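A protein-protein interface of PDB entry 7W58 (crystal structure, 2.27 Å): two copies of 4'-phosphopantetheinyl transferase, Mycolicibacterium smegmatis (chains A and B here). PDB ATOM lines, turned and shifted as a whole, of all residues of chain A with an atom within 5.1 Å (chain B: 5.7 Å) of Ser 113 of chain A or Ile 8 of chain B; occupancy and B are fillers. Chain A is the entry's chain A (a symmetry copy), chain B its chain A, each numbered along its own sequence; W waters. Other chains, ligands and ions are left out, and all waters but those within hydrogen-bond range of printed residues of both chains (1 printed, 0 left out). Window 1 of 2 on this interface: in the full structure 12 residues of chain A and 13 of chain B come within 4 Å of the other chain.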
ATOM      1  N   ILE A   8      10.807 -26.507 -11.042  1.00  0.00           N
ATOM      2  CA  ILE A   8       9.597 -26.880 -11.752  1.00  0.00           C
ATOM      3  C   ILE A   8       9.288 -28.338 -11.398  1.00  0.00           C
ATOM      4  O   ILE A   8      10.195 -29.114 -11.100  1.00  0.00           O
ATOM      5  CB  ILE A   8       9.735 -26.595 -13.266  1.00  0.00           C
ATOM      6  CG1 ILE A   8       8.420 -26.806 -14.028  1.00  0.00           C
ATOM      7  CG2 ILE A   8      10.898 -27.369 -13.885  1.00  0.00           C
ATOM      8  CD1 ILE A   8       8.461 -26.357 -15.475  1.00  0.00           C
ATOM      9  N   PRO A  93      -1.961 -20.287  -4.665  1.00  0.00           N
ATOM     10  CA  PRO A  93      -1.080 -20.877  -3.661  1.00  0.00           C
ATOM     11  C   PRO A  93      -0.381 -19.835  -2.790  1.00  0.00           C
ATOM     12  O   PRO A  93      -0.180 -18.692  -3.195  1.00  0.00           O
ATOM     13  CB  PRO A  93      -0.064 -21.643  -4.517  1.00  0.00           C
ATOM     14  CG  PRO A  93       0.033 -20.810  -5.766  1.00  0.00           C
ATOM     15  CD  PRO A  93      -1.384 -20.339  -6.015  1.00  0.00           C
ATOM     16  N   HIS A 111       8.235 -17.112  -4.771  1.00  0.00           N
ATOM     17  CA  HIS A 111       7.144 -17.023  -5.726  1.00  0.00           C
ATOM     18  C   HIS A 111       6.789 -18.436  -6.165  1.00  0.00           C
ATOM     19  O   HIS A 111       7.687 -19.235  -6.443  1.00  0.00           O
ATOM     20  CB  HIS A 111       7.551 -16.208  -6.963  1.00  0.00           C
ATOM     21  CG  HIS A 111       8.251 -14.930  -6.658  1.00  0.00           C
ATOM     22  ND1 HIS A 111       7.568 -13.753  -6.419  1.00  0.00           N
ATOM     23  CD2 HIS A 111       9.563 -14.638  -6.544  1.00  0.00           C
ATOM     24  CE1 HIS A 111       8.431 -12.788  -6.189  1.00  0.00           C
ATOM     25  NE2 HIS A 111       9.662 -13.305  -6.260  1.00  0.00           N
ATOM     26  N   VAL A 112       5.482 -18.710  -6.267  1.00  0.00           N
ATOM     27  CA  VAL A 112       4.997 -20.030  -6.633  1.00  0.00           C
ATOM     28  C   VAL A 112       3.759 -19.870  -7.505  1.00  0.00           C
ATOM     29  O   VAL A 112       2.944 -18.991  -7.253  1.00  0.00           O
ATOM     30  CB  VAL A 112       4.676 -20.857  -5.373  1.00  0.00           C
ATOM     31  CG1 VAL A 112       3.522 -20.254  -4.587  1.00  0.00           C
ATOM     32  CG2 VAL A 112       4.394 -22.318  -5.704  1.00  0.00           C
ATOM     33  N   SER A 113       3.634 -20.727  -8.525  1.00  0.00           N
ATOM     34  CA  SER A 113       2.411 -20.839  -9.305  1.00  0.00           C
ATOM     35  C   SER A 113       2.145 -22.317  -9.581  1.00  0.00           C
ATOM     36  O   SER A 113       3.097 -23.074  -9.744  1.00  0.00           O
ATOM     37  CB  SER A 113       2.491 -20.020 -10.582  1.00  0.00           C
ATOM     38  OG  SER A 113       1.245 -20.042 -11.269  1.00  0.00           O
ATOM     39  N   LEU A 114       0.860 -22.713  -9.590  1.00  0.00           N
ATOM     40  CA  LEU A 114       0.450 -24.084  -9.853  1.00  0.00           C
ATOM     41  C   LEU A 114      -0.709 -24.100 -10.851  1.00  0.00           C
ATOM     42  O   LEU A 114      -1.389 -23.101 -11.051  1.00  0.00           O
ATOM     43  CB  LEU A 114       0.095 -24.831  -8.551  1.00  0.00           C
ATOM     44  CG  LEU A 114      -0.869 -24.146  -7.568  1.00  0.00           C
ATOM     45  CD1 LEU A 114      -2.289 -24.046  -8.115  1.00  0.00           C
ATOM     46  CD2 LEU A 114      -0.887 -24.887  -6.242  1.00  0.00           C
ATOM     47  N   THR A 115      -0.930 -25.268 -11.460  1.00  0.00           N
ATOM     48  CA  THR A 115      -1.923 -25.473 -12.497  1.00  0.00           C
ATOM     49  C   THR A 115      -2.128 -26.975 -12.655  1.00  0.00           C
ATOM     50  O   THR A 115      -1.303 -27.773 -12.209  1.00  0.00           O
ATOM     51  CB  THR A 115      -1.405 -24.924 -13.833  1.00  0.00           C
ATOM     52  OG1 THR A 115      -2.404 -25.073 -14.841  1.00  0.00           O
ATOM     53  CG2 THR A 115      -0.151 -25.633 -14.301  1.00  0.00           C
ATOM     54  N   ALA A 122       1.196 -29.319 -12.466  1.00  0.00           N
ATOM     55  CA  ALA A 122       2.508 -28.694 -12.540  1.00  0.00           C
ATOM     56  C   ALA A 122       2.558 -27.448 -11.658  1.00  0.00           C
ATOM     57  O   ALA A 122       1.528 -26.883 -11.283  1.00  0.00           O
ATOM     58  CB  ALA A 122       2.881 -28.381 -13.974  1.00  0.00           C
ATOM     59  N   ALA A 123       3.791 -27.038 -11.338  1.00  0.00           N
ATOM     60  CA  ALA A 123       4.032 -25.835 -10.562  1.00  0.00           C
ATOM     61  C   ALA A 123       5.420 -25.274 -10.882  1.00  0.00           C
ATOM     62  O   ALA A 123       6.314 -26.003 -11.320  1.00  0.00           O
ATOM     63  CB  ALA A 123       3.906 -26.160  -9.100  1.00  0.00           C
ATOM     64  N   VAL A 124       5.600 -23.973 -10.632  1.00  0.00           N
ATOM     65  CA  VAL A 124       6.916 -23.368 -10.736  1.00  0.00           C
ATOM     66  C   VAL A 124       7.152 -22.588  -9.448  1.00  0.00           C
ATOM     67  O   VAL A 124       6.211 -22.044  -8.868  1.00  0.00           O
ATOM     68  CB  VAL A 124       7.024 -22.483 -11.995  1.00  0.00           C
ATOM     69  CG1 VAL A 124       6.119 -21.257 -11.912  1.00  0.00           C
ATOM     70  CG2 VAL A 124       8.456 -22.075 -12.297  1.00  0.00           C
ATOM     71  N   VAL B   6       4.407 -14.188 -10.903  1.00  0.00           N
ATOM     72  CA  VAL B   6       4.776 -15.387 -11.634  1.00  0.00           C
ATOM     73  C   VAL B   6       3.515 -16.206 -11.908  1.00  0.00           C
ATOM     74  O   VAL B   6       2.610 -16.269 -11.074  1.00  0.00           O
ATOM     75  CB  VAL B   6       5.830 -16.214 -10.869  1.00  0.00           C
ATOM     76  CG1 VAL B   6       6.090 -17.542 -11.555  1.00  0.00           C
ATOM     77  CG2 VAL B   6       7.140 -15.449 -10.721  1.00  0.00           C
ATOM     78  N   GLY B   7       3.485 -16.839 -13.089  1.00  0.00           N
ATOM     79  CA  GLY B   7       2.344 -17.621 -13.531  1.00  0.00           C
ATOM     80  C   GLY B   7       2.779 -18.789 -14.415  1.00  0.00           C
ATOM     81  O   GLY B   7       3.668 -18.649 -15.259  1.00  0.00           O
ATOM     82  N   ILE B   8       2.141 -19.939 -14.197  1.00  0.00           N
ATOM     83  CA  ILE B   8       2.300 -21.093 -15.064  1.00  0.00           C
ATOM     84  C   ILE B   8       0.899 -21.604 -15.411  1.00  0.00           C
ATOM     85  O   ILE B   8      -0.037 -21.436 -14.629  1.00  0.00           O
ATOM     86  CB  ILE B   8       3.233 -22.144 -14.419  1.00  0.00           C
ATOM     87  CG1 ILE B   8       3.573 -23.296 -15.374  1.00  0.00           C
ATOM     88  CG2 ILE B   8       2.692 -22.638 -13.079  1.00  0.00           C
ATOM     89  CD1 ILE B   8       4.631 -24.247 -14.850  1.00  0.00           C
ATOM     90  N   ASP B   9       0.731 -22.138 -16.626  1.00  0.00           N
ATOM     91  CA  ASP B   9      -0.550 -22.705 -17.016  1.00  0.00           C
ATOM     92  C   ASP B   9      -0.347 -23.927 -17.906  1.00  0.00           C
ATOM     93  O   ASP B   9       0.489 -23.916 -18.807  1.00  0.00           O
ATOM     94  CB  ASP B   9      -1.468 -21.676 -17.680  1.00  0.00           C
ATOM     95  CG  ASP B   9      -2.908 -22.163 -17.728  1.00  0.00           C
ATOM     96  OD1 ASP B   9      -3.419 -22.589 -16.677  1.00  0.00           O
ATOM     97  OD2 ASP B   9      -3.492 -22.162 -18.820  1.00  0.00           O
ATOM     98  N   LEU B  10      -1.136 -24.966 -17.630  1.00  0.00           N
ATOM     99  CA  LEU B  10      -1.177 -26.208 -18.383  1.00  0.00           C
ATOM    100  C   LEU B  10      -2.565 -26.378 -18.998  1.00  0.00           C
ATOM    101  O   LEU B  10      -3.581 -26.261 -18.315  1.00  0.00           O
ATOM    102  CB  LEU B  10      -0.924 -27.321 -17.369  1.00  0.00           C
ATOM    103  CG  LEU B  10      -0.420 -28.656 -17.899  1.00  0.00           C
ATOM    104  CD1 LEU B  10       0.968 -28.521 -18.502  1.00  0.00           C
ATOM    105  CD2 LEU B  10      -0.383 -29.641 -16.743  1.00  0.00           C
ATOM    106  N   ALA B  55      -2.523 -20.768 -23.131  1.00  0.00           N
ATOM    107  CA  ALA B  55      -1.772 -21.034 -21.907  1.00  0.00           C
ATOM    108  C   ALA B  55      -0.931 -19.820 -21.512  1.00  0.00           C
ATOM    109  O   ALA B  55      -0.769 -19.529 -20.321  1.00  0.00           O
ATOM    110  CB  ALA B  55      -0.890 -22.243 -22.082  1.00  0.00           C
ATOM    111  N   ALA B  59      -1.186 -17.746 -18.192  1.00  0.00           N
ATOM    112  CA  ALA B  59      -0.016 -17.585 -17.342  1.00  0.00           C
ATOM    113  C   ALA B  59       0.203 -16.100 -16.996  1.00  0.00           C
ATOM    114  O   ALA B  59       0.440 -15.762 -15.836  1.00  0.00           O
ATOM    115  CB  ALA B  59       1.187 -18.247 -17.974  1.00  0.00           C
ATOM    116  N   LYS B  62      -2.407 -14.922 -14.481  1.00  0.00           N
ATOM    117  CA  LYS B  62      -2.111 -15.458 -13.154  1.00  0.00           C
ATOM    118  C   LYS B  62      -1.033 -14.619 -12.462  1.00  0.00           C
ATOM    119  O   LYS B  62      -1.181 -14.261 -11.294  1.00  0.00           O
ATOM    120  CB  LYS B  62      -1.753 -16.947 -13.215  1.00  0.00           C
ATOM    121  CG  LYS B  62      -2.928 -17.898 -13.017  1.00  0.00           C
ATOM    122  CD  LYS B  62      -2.782 -19.244 -13.709  1.00  0.00           C
ATOM    123  CE  LYS B  62      -2.620 -20.435 -12.786  1.00  0.00           C
ATOM    124  NZ  LYS B  62      -2.884 -21.711 -13.507  1.00  0.00           N
ATOM    125  N   ALA B 123       2.724 -22.734 -20.636  1.00  0.00           N
ATOM    126  CA  ALA B 123       3.387 -21.446 -20.736  1.00  0.00           C
ATOM    127  C   ALA B 123       3.847 -20.983 -19.352  1.00  0.00           C
ATOM    128  O   ALA B 123       3.295 -21.397 -18.328  1.00  0.00           O
ATOM    129  CB  ALA B 123       2.441 -20.452 -21.350  1.00  0.00           C
ATOM    130  N   VAL B 124       4.847 -20.098 -19.330  1.00  0.00           N
ATOM    131  CA  VAL B 124       5.255 -19.462 -18.090  1.00  0.00           C
ATOM    132  C   VAL B 124       5.313 -17.962 -18.356  1.00  0.00           C
ATOM    133  O   VAL B 124       5.642 -17.537 -19.463  1.00  0.00           O
ATOM    134  CB  VAL B 124       6.601 -20.028 -17.589  1.00  0.00           C
ATOM    135  CG1 VAL B 124       7.755 -19.669 -18.522  1.00  0.00           C
ATOM    136  CG2 VAL B 124       6.912 -19.609 -16.163  1.00  0.00           C
ATOM    137  N   ALA B 125       4.927 -17.174 -17.350  1.00  0.00           N
ATOM    138  CA  ALA B 125       5.028 -15.730 -17.427  1.00  0.00           C
ATOM    139  C   ALA B 125       5.688 -15.199 -16.162  1.00  0.00           C
ATOM    140  O   ALA B 125       5.355 -15.621 -15.047  1.00  0.00           O
ATOM    141  CB  ALA B 125       3.663 -15.136 -17.632  1.00  0.00           C
HETATM  142  O   HOH W   1      -5.083 -24.376 -16.167  1.00  0.00           O
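Val 124 of chain A touches Ile 8 of chain B, but with the chains exchanged Ile 8 of chain A does not touch Val 124 of chain B (6.9 Å).
Of the 12 pairs that touch across the chains among the printed residues, none has its exchanged pair printed and touching as well.
Water W1 lies within hydrogen-bond range of OD1 of Asp 9 of chain B, OG1 of Thr 115 of chain A and O of Leu 10 of chain B.
His 111 of chain A touches Val 6 of chain B (CB to CG2, 3.9 Å).
Val 6 of chain B touches Ser 113 of chain A.
CA of Gly 7 of chain B touches OG of Ser 113 of chain A, 3.5 Å away.
Leu 114 of chain A touches Ile 8 of chain B (N to CG2, 3.9 Å).
Thr 115 of chain A touches Ile 8 of chain B (CB to O, 3.8 Å).
Thr 115 of chain A touches Lys 62 of chain B.
Val 124 of chain A touches Val 6 of chain B.
Ile 8 of chain B touches Val 124 of chain A (CG2 to CG1, 3.9 Å).
Printed residues of chain B that touch a printed residue of chain A: Val 6, Gly 7, Ile 8, Asp 9, Leu 10 and Lys 62.
Of the 10 printed residues of chain A, 5 touch a printed residue of chain B.
Among the printed residues, 12 pairs touch across the chains.
Among the printed residues, no Asp or Glu carboxylate lies within 4 Å of a Lys or Arg side-chain nitrogen of the other chain.
The side-chain hydroxyl (OG1) of Thr 115 of chain A lies within hydrogen-bond range of the side-chain carboxylate (OD1) of Asp 9 of chain B (3.3 Å).
OG of Ser 113 of chain A is in hydrogen-bond range of N of Ile 8 of chain B, 3.1 Å away.
OG1 of Thr 115 of chain A sits at hydrogen-bond distance from N of Leu 10 of chain B (3.1 Å).
The backbone carbonyl oxygen (O) of Leu 114 of chain A sits at hydrogen-bond distance from the side-chain amino group (NZ) of Lys 62 of chain B (3.2 Å).
The side-chain amino group of Lys 62 of chain B is in hydrogen-bond range of the backbone carbonyl oxygen of Ile 8 of chain B (3.1 Å).
The backbone carbonyl oxygen (O) of Asp 9 of chain B is in hydrogen-bond range of the backbone NH (N) of Ala 123 of chain B (3.1 Å).
N of Val 124 of chain A sits at hydrogen-bond distance from O of Ser 113 of chain A (2.8 Å).
NZ of Lys 62 of chain B lies within salt-bridge range of OD1 of Asp 9 of chain B.
N of Ala 125 of chain B sits at hydrogen-bond distance from O of Gly 7 of chain B, 2.9 Å away.
N of Thr 115 of chain A is in hydrogen-bond range of O of Ala 122 of chain A (2.9 Å).
Of chain B, only Val 6, Gly 7 and Ile 8 come within 4 Å of Ser 113 of chain A.
Printed residues of chain B within 4 Å of Leu 114 of chain A: Ile 8 and Lys 62.
Printed residues of chain B within 4 Å of Thr 115 of chain A: Ile 8, Asp 9, Leu 10 and Lys 62.
Of the printed residues of chain B, Val 124 of chain A touches Val 6 (3.7 Å) and Ile 8 (3.9 Å).
Of chain A, only Ser 113 (3.1 Å), Leu 114 (3.9 Å), Thr 115 (3.8 Å) and Val 124 (3.9 Å) come within 4 Å of Ile 8 of chain B.
Of the printed residues of chain A, Asp 9 of chain B touches Thr 115 (3.3 Å).
The nearest residue of chain A that does not touch Ile 8 of chain B is Ala 123 of chain A (4.2 Å).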
